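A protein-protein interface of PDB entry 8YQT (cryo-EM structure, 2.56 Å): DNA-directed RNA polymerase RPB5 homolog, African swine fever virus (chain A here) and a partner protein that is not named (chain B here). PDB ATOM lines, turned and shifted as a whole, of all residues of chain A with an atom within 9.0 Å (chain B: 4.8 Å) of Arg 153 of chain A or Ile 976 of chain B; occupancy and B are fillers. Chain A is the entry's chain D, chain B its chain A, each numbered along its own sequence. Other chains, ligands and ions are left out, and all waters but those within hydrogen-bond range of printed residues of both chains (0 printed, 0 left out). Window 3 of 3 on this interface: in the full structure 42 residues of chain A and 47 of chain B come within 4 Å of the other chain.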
ATOM      1  N   GLU A 145     -15.315  -7.511   0.246  1.00  0.00           N
ATOM      2  CA  GLU A 145     -14.193  -6.595   0.433  1.00  0.00           C
ATOM      3  C   GLU A 145     -13.698  -6.036  -0.897  1.00  0.00           C
ATOM      4  O   GLU A 145     -13.438  -4.832  -1.013  1.00  0.00           O
ATOM      5  CB  GLU A 145     -13.064  -7.305   1.176  1.00  0.00           C
ATOM      6  CG  GLU A 145     -12.004  -6.375   1.728  1.00  0.00           C
ATOM      7  CD  GLU A 145     -10.600  -6.820   1.379  1.00  0.00           C
ATOM      8  OE1 GLU A 145      -9.650  -6.372   2.056  1.00  0.00           O
ATOM      9  OE2 GLU A 145     -10.445  -7.615   0.429  1.00  0.00           O
ATOM     10  N   GLU A 146     -13.560  -6.894  -1.913  1.00  0.00           N
ATOM     11  CA  GLU A 146     -13.156  -6.419  -3.233  1.00  0.00           C
ATOM     12  C   GLU A 146     -14.194  -5.483  -3.831  1.00  0.00           C
ATOM     13  O   GLU A 146     -13.838  -4.461  -4.428  1.00  0.00           O
ATOM     14  CB  GLU A 146     -12.921  -7.599  -4.172  1.00  0.00           C
ATOM     15  CG  GLU A 146     -11.726  -8.459  -3.821  1.00  0.00           C
ATOM     16  CD  GLU A 146     -11.606  -9.673  -4.723  1.00  0.00           C
ATOM     17  OE1 GLU A 146     -12.650 -10.181  -5.180  1.00  0.00           O
ATOM     18  OE2 GLU A 146     -10.466 -10.116  -4.976  1.00  0.00           O
ATOM     19  N   ALA A 147     -15.476  -5.820  -3.686  1.00  0.00           N
ATOM     20  CA  ALA A 147     -16.530  -4.950  -4.190  1.00  0.00           C
ATOM     21  C   ALA A 147     -16.536  -3.617  -3.460  1.00  0.00           C
ATOM     22  O   ALA A 147     -16.768  -2.571  -4.073  1.00  0.00           O
ATOM     23  CB  ALA A 147     -17.885  -5.640  -4.062  1.00  0.00           C
ATOM     24  N   GLN A 148     -16.290  -3.635  -2.149  1.00  0.00           N
ATOM     25  CA  GLN A 148     -16.208  -2.391  -1.396  1.00  0.00           C
ATOM     26  C   GLN A 148     -15.036  -1.535  -1.855  1.00  0.00           C
ATOM     27  O   GLN A 148     -15.181  -0.317  -1.985  1.00  0.00           O
ATOM     28  CB  GLN A 148     -16.101  -2.686   0.099  1.00  0.00           C
ATOM     29  CG  GLN A 148     -17.105  -1.928   0.949  1.00  0.00           C
ATOM     30  CD  GLN A 148     -18.539  -2.288   0.617  1.00  0.00           C
ATOM     31  OE1 GLN A 148     -18.947  -3.442   0.742  1.00  0.00           O
ATOM     32  NE2 GLN A 148     -19.314  -1.298   0.186  1.00  0.00           N
ATOM     33  N   GLU A 149     -13.879  -2.148  -2.110  1.00  0.00           N
ATOM     34  CA  GLU A 149     -12.742  -1.390  -2.629  1.00  0.00           C
ATOM     35  C   GLU A 149     -13.056  -0.783  -3.994  1.00  0.00           C
ATOM     36  O   GLU A 149     -12.758   0.394  -4.245  1.00  0.00           O
ATOM     37  CB  GLU A 149     -11.510  -2.291  -2.710  1.00  0.00           C
ATOM     38  CG  GLU A 149     -10.183  -1.551  -2.786  1.00  0.00           C
ATOM     39  CD  GLU A 149      -9.697  -1.048  -1.438  1.00  0.00           C
ATOM     40  OE1 GLU A 149      -8.554  -0.550  -1.367  1.00  0.00           O
ATOM     41  OE2 GLU A 149     -10.451  -1.152  -0.446  1.00  0.00           O
ATOM     42  N   PHE A 150     -13.670  -1.570  -4.882  1.00  0.00           N
ATOM     43  CA  PHE A 150     -14.040  -1.066  -6.201  1.00  0.00           C
ATOM     44  C   PHE A 150     -15.018   0.097  -6.095  1.00  0.00           C
ATOM     45  O   PHE A 150     -14.848   1.127  -6.755  1.00  0.00           O
ATOM     46  CB  PHE A 150     -14.638  -2.194  -7.042  1.00  0.00           C
ATOM     47  CG  PHE A 150     -15.370  -1.715  -8.260  1.00  0.00           C
ATOM     48  CD1 PHE A 150     -14.676  -1.286  -9.375  1.00  0.00           C
ATOM     49  CD2 PHE A 150     -16.752  -1.684  -8.286  1.00  0.00           C
ATOM     50  CE1 PHE A 150     -15.347  -0.842 -10.492  1.00  0.00           C
ATOM     51  CE2 PHE A 150     -17.424  -1.239  -9.399  1.00  0.00           C
ATOM     52  CZ  PHE A 150     -16.719  -0.817 -10.503  1.00  0.00           C
ATOM     53  N   LEU A 151     -16.053  -0.051  -5.266  1.00  0.00           N
ATOM     54  CA  LEU A 151     -17.047   1.004  -5.107  1.00  0.00           C
ATOM     55  C   LEU A 151     -16.449   2.249  -4.469  1.00  0.00           C
ATOM     56  O   LEU A 151     -16.845   3.368  -4.812  1.00  0.00           O
ATOM     57  CB  LEU A 151     -18.221   0.498  -4.271  1.00  0.00           C
ATOM     58  CG  LEU A 151     -19.167  -0.513  -4.914  1.00  0.00           C
ATOM     59  CD1 LEU A 151     -20.069  -1.126  -3.866  1.00  0.00           C
ATOM     60  CD2 LEU A 151     -19.987   0.140  -6.004  1.00  0.00           C
ATOM     61  N   GLY A 152     -15.512   2.078  -3.536  1.00  0.00           N
ATOM     62  CA  GLY A 152     -14.863   3.226  -2.935  1.00  0.00           C
ATOM     63  C   GLY A 152     -14.010   3.995  -3.923  1.00  0.00           C
ATOM     64  O   GLY A 152     -13.998   5.228  -3.913  1.00  0.00           O
ATOM     65  N   ARG A 153     -13.281   3.282  -4.785  1.00  0.00           N
ATOM     66  CA  ARG A 153     -12.500   3.973  -5.807  1.00  0.00           C
ATOM     67  C   ARG A 153     -13.394   4.736  -6.778  1.00  0.00           C
ATOM     68  O   ARG A 153     -12.997   5.790  -7.284  1.00  0.00           O
ATOM     69  CB  ARG A 153     -11.620   2.980  -6.565  1.00  0.00           C
ATOM     70  CG  ARG A 153     -10.552   3.631  -7.429  1.00  0.00           C
ATOM     71  CD  ARG A 153     -10.961   3.676  -8.892  1.00  0.00           C
ATOM     72  NE  ARG A 153      -9.966   4.347  -9.719  1.00  0.00           N
ATOM     73  CZ  ARG A 153     -10.186   4.771 -10.956  1.00  0.00           C
ATOM     74  NH1 ARG A 153     -11.357   4.604 -11.546  1.00  0.00           N
ATOM     75  NH2 ARG A 153      -9.206   5.378 -11.618  1.00  0.00           N
ATOM     76  N   GLU A 154     -14.595   4.231  -7.039  1.00  0.00           N
ATOM     77  CA  GLU A 154     -15.500   4.798  -8.028  1.00  0.00           C
ATOM     78  C   GLU A 154     -16.476   5.812  -7.447  1.00  0.00           C
ATOM     79  O   GLU A 154     -17.258   6.390  -8.206  1.00  0.00           O
ATOM     80  CB  GLU A 154     -16.290   3.678  -8.711  1.00  0.00           C
ATOM     81  CG  GLU A 154     -15.439   2.669  -9.453  1.00  0.00           C
ATOM     82  CD  GLU A 154     -14.995   3.160 -10.810  1.00  0.00           C
ATOM     83  OE1 GLU A 154     -15.828   3.743 -11.532  1.00  0.00           O
ATOM     84  OE2 GLU A 154     -13.811   2.967 -11.154  1.00  0.00           O
ATOM     85  N   TYR A 155     -16.449   6.039  -6.133  1.00  0.00           N
ATOM     86  CA  TYR A 155     -17.416   6.898  -5.450  1.00  0.00           C
ATOM     87  C   TYR A 155     -18.848   6.468  -5.761  1.00  0.00           C
ATOM     88  O   TYR A 155     -19.707   7.277  -6.113  1.00  0.00           O
ATOM     89  CB  TYR A 155     -17.200   8.370  -5.803  1.00  0.00           C
ATOM     90  CG  TYR A 155     -16.079   9.037  -5.043  1.00  0.00           C
ATOM     91  CD1 TYR A 155     -16.267   9.486  -3.744  1.00  0.00           C
ATOM     92  CD2 TYR A 155     -14.837   9.228  -5.625  1.00  0.00           C
ATOM     93  CE1 TYR A 155     -15.250  10.096  -3.049  1.00  0.00           C
ATOM     94  CE2 TYR A 155     -13.814   9.838  -4.935  1.00  0.00           C
ATOM     95  CZ  TYR A 155     -14.026  10.271  -3.648  1.00  0.00           C
ATOM     96  OH  TYR A 155     -13.007  10.881  -2.958  1.00  0.00           O
ATOM     97  N   LEU A 156     -19.104   5.172  -5.625  1.00  0.00           N
ATOM     98  CA  LEU A 156     -20.391   4.594  -5.969  1.00  0.00           C
ATOM     99  C   LEU A 156     -21.000   3.882  -4.770  1.00  0.00           C
ATOM    100  O   LEU A 156     -20.304   3.460  -3.844  1.00  0.00           O
ATOM    101  CB  LEU A 156     -20.267   3.604  -7.135  1.00  0.00           C
ATOM    102  CG  LEU A 156     -20.088   4.145  -8.553  1.00  0.00           C
ATOM    103  CD1 LEU A 156     -19.794   3.006  -9.503  1.00  0.00           C
ATOM    104  CD2 LEU A 156     -21.322   4.901  -8.996  1.00  0.00           C
ATOM    105  N   TYR B 841     -15.765   9.499 -15.054  1.00  0.00           N
ATOM    106  CA  TYR B 841     -15.051   8.231 -15.117  1.00  0.00           C
ATOM    107  C   TYR B 841     -15.147   7.586 -16.493  1.00  0.00           C
ATOM    108  O   TYR B 841     -14.749   6.429 -16.655  1.00  0.00           O
ATOM    109  CB  TYR B 841     -15.572   7.268 -14.052  1.00  0.00           C
ATOM    110  CG  TYR B 841     -15.225   7.642 -12.634  1.00  0.00           C
ATOM    111  CD1 TYR B 841     -15.938   8.616 -11.954  1.00  0.00           C
ATOM    112  CD2 TYR B 841     -14.190   7.006 -11.971  1.00  0.00           C
ATOM    113  CE1 TYR B 841     -15.621   8.952 -10.658  1.00  0.00           C
ATOM    114  CE2 TYR B 841     -13.869   7.333 -10.678  1.00  0.00           C
ATOM    115  CZ  TYR B 841     -14.585   8.306 -10.026  1.00  0.00           C
ATOM    116  OH  TYR B 841     -14.255   8.628  -8.733  1.00  0.00           O
ATOM    117  N   PRO B 972      -3.018   1.881 -19.809  1.00  0.00           N
ATOM    118  CA  PRO B 972      -4.339   2.219 -19.252  1.00  0.00           C
ATOM    119  C   PRO B 972      -4.392   3.549 -18.519  1.00  0.00           C
ATOM    120  O   PRO B 972      -5.496   4.039 -18.259  1.00  0.00           O
ATOM    121  CB  PRO B 972      -4.626   1.055 -18.298  1.00  0.00           C
ATOM    122  CG  PRO B 972      -3.808  -0.045 -18.799  1.00  0.00           C
ATOM    123  CD  PRO B 972      -2.555   0.583 -19.289  1.00  0.00           C
ATOM    124  N   TYR B 973      -3.252   4.146 -18.170  1.00  0.00           N
ATOM    125  CA  TYR B 973      -3.252   5.467 -17.553  1.00  0.00           C
ATOM    126  C   TYR B 973      -3.716   6.559 -18.499  1.00  0.00           C
ATOM    127  O   TYR B 973      -3.940   7.685 -18.046  1.00  0.00           O
ATOM    128  CB  TYR B 973      -1.863   5.809 -17.017  1.00  0.00           C
ATOM    129  CG  TYR B 973      -1.497   5.055 -15.763  1.00  0.00           C
ATOM    130  CD1 TYR B 973      -2.241   5.200 -14.605  1.00  0.00           C
ATOM    131  CD2 TYR B 973      -0.403   4.206 -15.736  1.00  0.00           C
ATOM    132  CE1 TYR B 973      -1.913   4.519 -13.458  1.00  0.00           C
ATOM    133  CE2 TYR B 973      -0.066   3.521 -14.592  1.00  0.00           C
ATOM    134  CZ  TYR B 973      -0.826   3.682 -13.457  1.00  0.00           C
ATOM    135  OH  TYR B 973      -0.499   3.000 -12.312  1.00  0.00           O
ATOM    136  N   VAL B 974      -3.852   6.265 -19.791  1.00  0.00           N
ATOM    137  CA  VAL B 974      -4.504   7.197 -20.704  1.00  0.00           C
ATOM    138  C   VAL B 974      -5.914   7.499 -20.217  1.00  0.00           C
ATOM    139  O   VAL B 974      -6.418   8.618 -20.370  1.00  0.00           O
ATOM    140  CB  VAL B 974      -4.499   6.622 -22.133  1.00  0.00           C
ATOM    141  CG1 VAL B 974      -5.433   7.398 -23.037  1.00  0.00           C
ATOM    142  CG2 VAL B 974      -3.096   6.631 -22.698  1.00  0.00           C
ATOM    143  N   PHE B 975      -6.559   6.516 -19.598  1.00  0.00           N
ATOM    144  CA  PHE B 975      -7.910   6.671 -19.087  1.00  0.00           C
ATOM    145  C   PHE B 975      -7.972   7.362 -17.734  1.00  0.00           C
ATOM    146  O   PHE B 975      -9.077   7.649 -17.266  1.00  0.00           O
ATOM    147  CB  PHE B 975      -8.595   5.307 -18.985  1.00  0.00           C
ATOM    148  CG  PHE B 975      -8.835   4.649 -20.306  1.00  0.00           C
ATOM    149  CD1 PHE B 975      -9.795   5.138 -21.170  1.00  0.00           C
ATOM    150  CD2 PHE B 975      -8.105   3.539 -20.683  1.00  0.00           C
ATOM    151  CE1 PHE B 975     -10.017   4.535 -22.383  1.00  0.00           C
ATOM    152  CE2 PHE B 975      -8.324   2.937 -21.894  1.00  0.00           C
ATOM    153  CZ  PHE B 975      -9.280   3.434 -22.745  1.00  0.00           C
ATOM    154  N   ILE B 976      -6.840   7.635 -17.080  1.00  0.00           N
ATOM    155  CA  ILE B 976      -6.929   8.296 -15.784  1.00  0.00           C
ATOM    156  C   ILE B 976      -6.301   9.683 -15.825  1.00  0.00           C
ATOM    157  O   ILE B 976      -7.017  10.681 -15.941  1.00  0.00           O
ATOM    158  CB  ILE B 976      -6.259   7.432 -14.702  1.00  0.00           C
ATOM    159  CG1 ILE B 976      -6.815   6.008 -14.744  1.00  0.00           C
ATOM    160  CG2 ILE B 976      -6.442   8.055 -13.332  1.00  0.00           C
ATOM    161  CD1 ILE B 976      -6.007   5.012 -13.966  1.00  0.00           C
ATOM    162  N   ASN B 977      -4.967   9.750 -15.812  1.00  0.00           N
ATOM    163  CA  ASN B 977      -4.205  10.991 -15.949  1.00  0.00           C
ATOM    164  C   ASN B 977      -2.717  10.700 -15.801  1.00  0.00           C
ATOM    165  O   ASN B 977      -2.332   9.564 -15.516  1.00  0.00           O
ATOM    166  CB  ASN B 977      -4.655  12.078 -14.955  1.00  0.00           C
ATOM    167  CG  ASN B 977      -4.471  11.691 -13.499  1.00  0.00           C
ATOM    168  OD1 ASN B 977      -3.504  11.040 -13.120  1.00  0.00           O
ATOM    169  ND2 ASN B 977      -5.409  12.114 -12.670  1.00  0.00           N
ATOM    170  N   GLN B 980      -1.407   9.947 -11.737  1.00  0.00           N
ATOM    171  CA  GLN B 980      -1.420   8.574 -11.256  1.00  0.00           C
ATOM    172  C   GLN B 980      -0.426   7.692 -11.992  1.00  0.00           C
ATOM    173  O   GLN B 980       0.063   6.718 -11.413  1.00  0.00           O
ATOM    174  CB  GLN B 980      -2.824   7.981 -11.375  1.00  0.00           C
ATOM    175  CG  GLN B 980      -3.917   8.862 -10.802  1.00  0.00           C
ATOM    176  CD  GLN B 980      -3.723   9.159  -9.330  1.00  0.00           C
ATOM    177  OE1 GLN B 980      -3.458   8.261  -8.535  1.00  0.00           O
ATOM    178  NE2 GLN B 980      -3.850  10.424  -8.960  1.00  0.00           N
ATOM    179  N   ILE B 987      -4.464   0.141 -11.112  1.00  0.00           N
ATOM    180  CA  ILE B 987      -5.378   0.422 -12.215  1.00  0.00           C
ATOM    181  C   ILE B 987      -6.617  -0.451 -12.058  1.00  0.00           C
ATOM    182  O   ILE B 987      -6.494  -1.645 -11.757  1.00  0.00           O
ATOM    183  CB  ILE B 987      -4.691   0.182 -13.569  1.00  0.00           C
ATOM    184  CG1 ILE B 987      -3.490   1.114 -13.727  1.00  0.00           C
ATOM    185  CG2 ILE B 987      -5.669   0.363 -14.721  1.00  0.00           C
ATOM    186  CD1 ILE B 987      -2.604   0.775 -14.892  1.00  0.00           C
ATOM    187  N   PRO B 988      -7.820   0.095 -12.235  1.00  0.00           N
ATOM    188  CA  PRO B 988      -9.019  -0.748 -12.206  1.00  0.00           C
ATOM    189  C   PRO B 988      -8.977  -1.813 -13.291  1.00  0.00           C
ATOM    190  O   PRO B 988      -8.421  -1.609 -14.372  1.00  0.00           O
ATOM    191  CB  PRO B 988     -10.158   0.247 -12.444  1.00  0.00           C
ATOM    192  CG  PRO B 988      -9.605   1.557 -12.031  1.00  0.00           C
ATOM    193  CD  PRO B 988      -8.151   1.522 -12.364  1.00  0.00           C
ATOM    194  N   TYR B 990     -11.371  -3.016 -15.115  1.00  0.00           N
ATOM    195  CA  TYR B 990     -12.119  -2.679 -16.319  1.00  0.00           C
ATOM    196  C   TYR B 990     -11.380  -1.690 -17.210  1.00  0.00           C
ATOM    197  O   TYR B 990     -11.732  -1.556 -18.384  1.00  0.00           O
ATOM    198  CB  TYR B 990     -13.502  -2.134 -15.954  1.00  0.00           C
ATOM    199  CG  TYR B 990     -13.528  -0.694 -15.502  1.00  0.00           C
ATOM    200  CD1 TYR B 990     -13.283  -0.359 -14.181  1.00  0.00           C
ATOM    201  CD2 TYR B 990     -13.815   0.329 -16.391  1.00  0.00           C
ATOM    202  CE1 TYR B 990     -13.312   0.952 -13.763  1.00  0.00           C
ATOM    203  CE2 TYR B 990     -13.844   1.641 -15.981  1.00  0.00           C
ATOM    204  CZ  TYR B 990     -13.593   1.947 -14.669  1.00  0.00           C
ATOM    205  OH  TYR B 990     -13.624   3.257 -14.256  1.00  0.00           O
ATOM    206  N   LEU B 991     -10.370  -0.994 -16.687  1.00  0.00           N
ATOM    207  CA  LEU B 991      -9.551  -0.114 -17.509  1.00  0.00           C
ATOM    208  C   LEU B 991      -8.371  -0.831 -18.144  1.00  0.00           C
ATOM    209  O   LEU B 991      -7.887  -0.391 -19.190  1.00  0.00           O
ATOM    210  CB  LEU B 991      -9.035   1.071 -16.689  1.00  0.00           C
ATOM    211  CG  LEU B 991     -10.061   2.128 -16.290  1.00  0.00           C
ATOM    212  CD1 LEU B 991      -9.392   3.240 -15.512  1.00  0.00           C
ATOM    213  CD2 LEU B 991     -10.769   2.675 -17.514  1.00  0.00           C
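OE2 of Glu 154 of chain A is in hydrogen-bond range of OH of Tyr 990 of chain B (3.1 Å).
The side-chain hydroxyl (OH) of Tyr 841 of chain B sits at hydrogen-bond distance from the backbone carbonyl oxygen (O) of Arg 153 of chain A, 3.4 Å away.
OE2 of Glu 154 of chain A is in salt-bridge range of NH1 of Arg 153 of chain A (3.0 Å).
Among the printed residues, pairs that only touch across the chains: Arg 153 of chain A with Ile 976 of chain B (3.99 Å), Arg 153 of chain A with Pro 988 of chain B (3.4 Å), Arg 153 of chain A with Tyr 990 of chain B (3.8 Å), Glu 154 of chain A with Tyr 841 of chain B (3.7 Å) and Tyr 155 of chain A with Tyr 841 of chain B (3.2 Å).
Of the printed residues of chain B, Arg 153 of chain A touches Tyr 841, Ile 976, Pro 988 and Tyr 990.
Printed residues of chain B within 4 Å of Glu 154 of chain A: Tyr 841 (3.7 Å) and Tyr 990 (3.1 Å).
Printed residues of chain A within 4 Å of Tyr 841 of chain B: Arg 153 (3.4 Å), Glu 154 (3.7 Å) and Tyr 155 (3.2 Å).
Pro 972 of chain B touches none of the printed residues of chain A.
Of the printed residues of chain A, Ile 976 of chain B touches Arg 153.
No residue of chain A comes within 4 Å of Asn 977 of chain B.
Gln 980 of chain B touches none of the printed residues of chain A.
Printed residues of chain A within 4 Å of Pro 988 of chain B: Arg 153.
The nearest printed residue of chain A that does not touch Pro 988 of chain B is Glu 154 of chain A (4.5 Å).
Of the 12 printed residues of chain A, 3 touch a printed residue of chain B.
Printed residues of chain A that touch a printed residue of chain B: Arg 153, Glu 154 and Tyr 155.
Hydrophobic or aromatic side chains of chain A within 4 Å of the printed part of chain B: Tyr 155.
Printed residues of chain B that touch a printed residue of chain A: Tyr 841, Ile 976, Pro 988 and Tyr 990.
Hydrophobic or aromatic side chains of chain B within 4 Å of the printed part of chain A: Tyr 841, Ile 976, Pro 988 and Tyr 990.
Along chain B the printed residues that touch a printed residue of chain A span positions 841 to 990.
Among the printed residues, 7 pairs touch across the chains.
Among the printed residues, no Asp or Glu carboxylate lies within 4 Å of a Lys or Arg side-chain nitrogen of the other chain.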
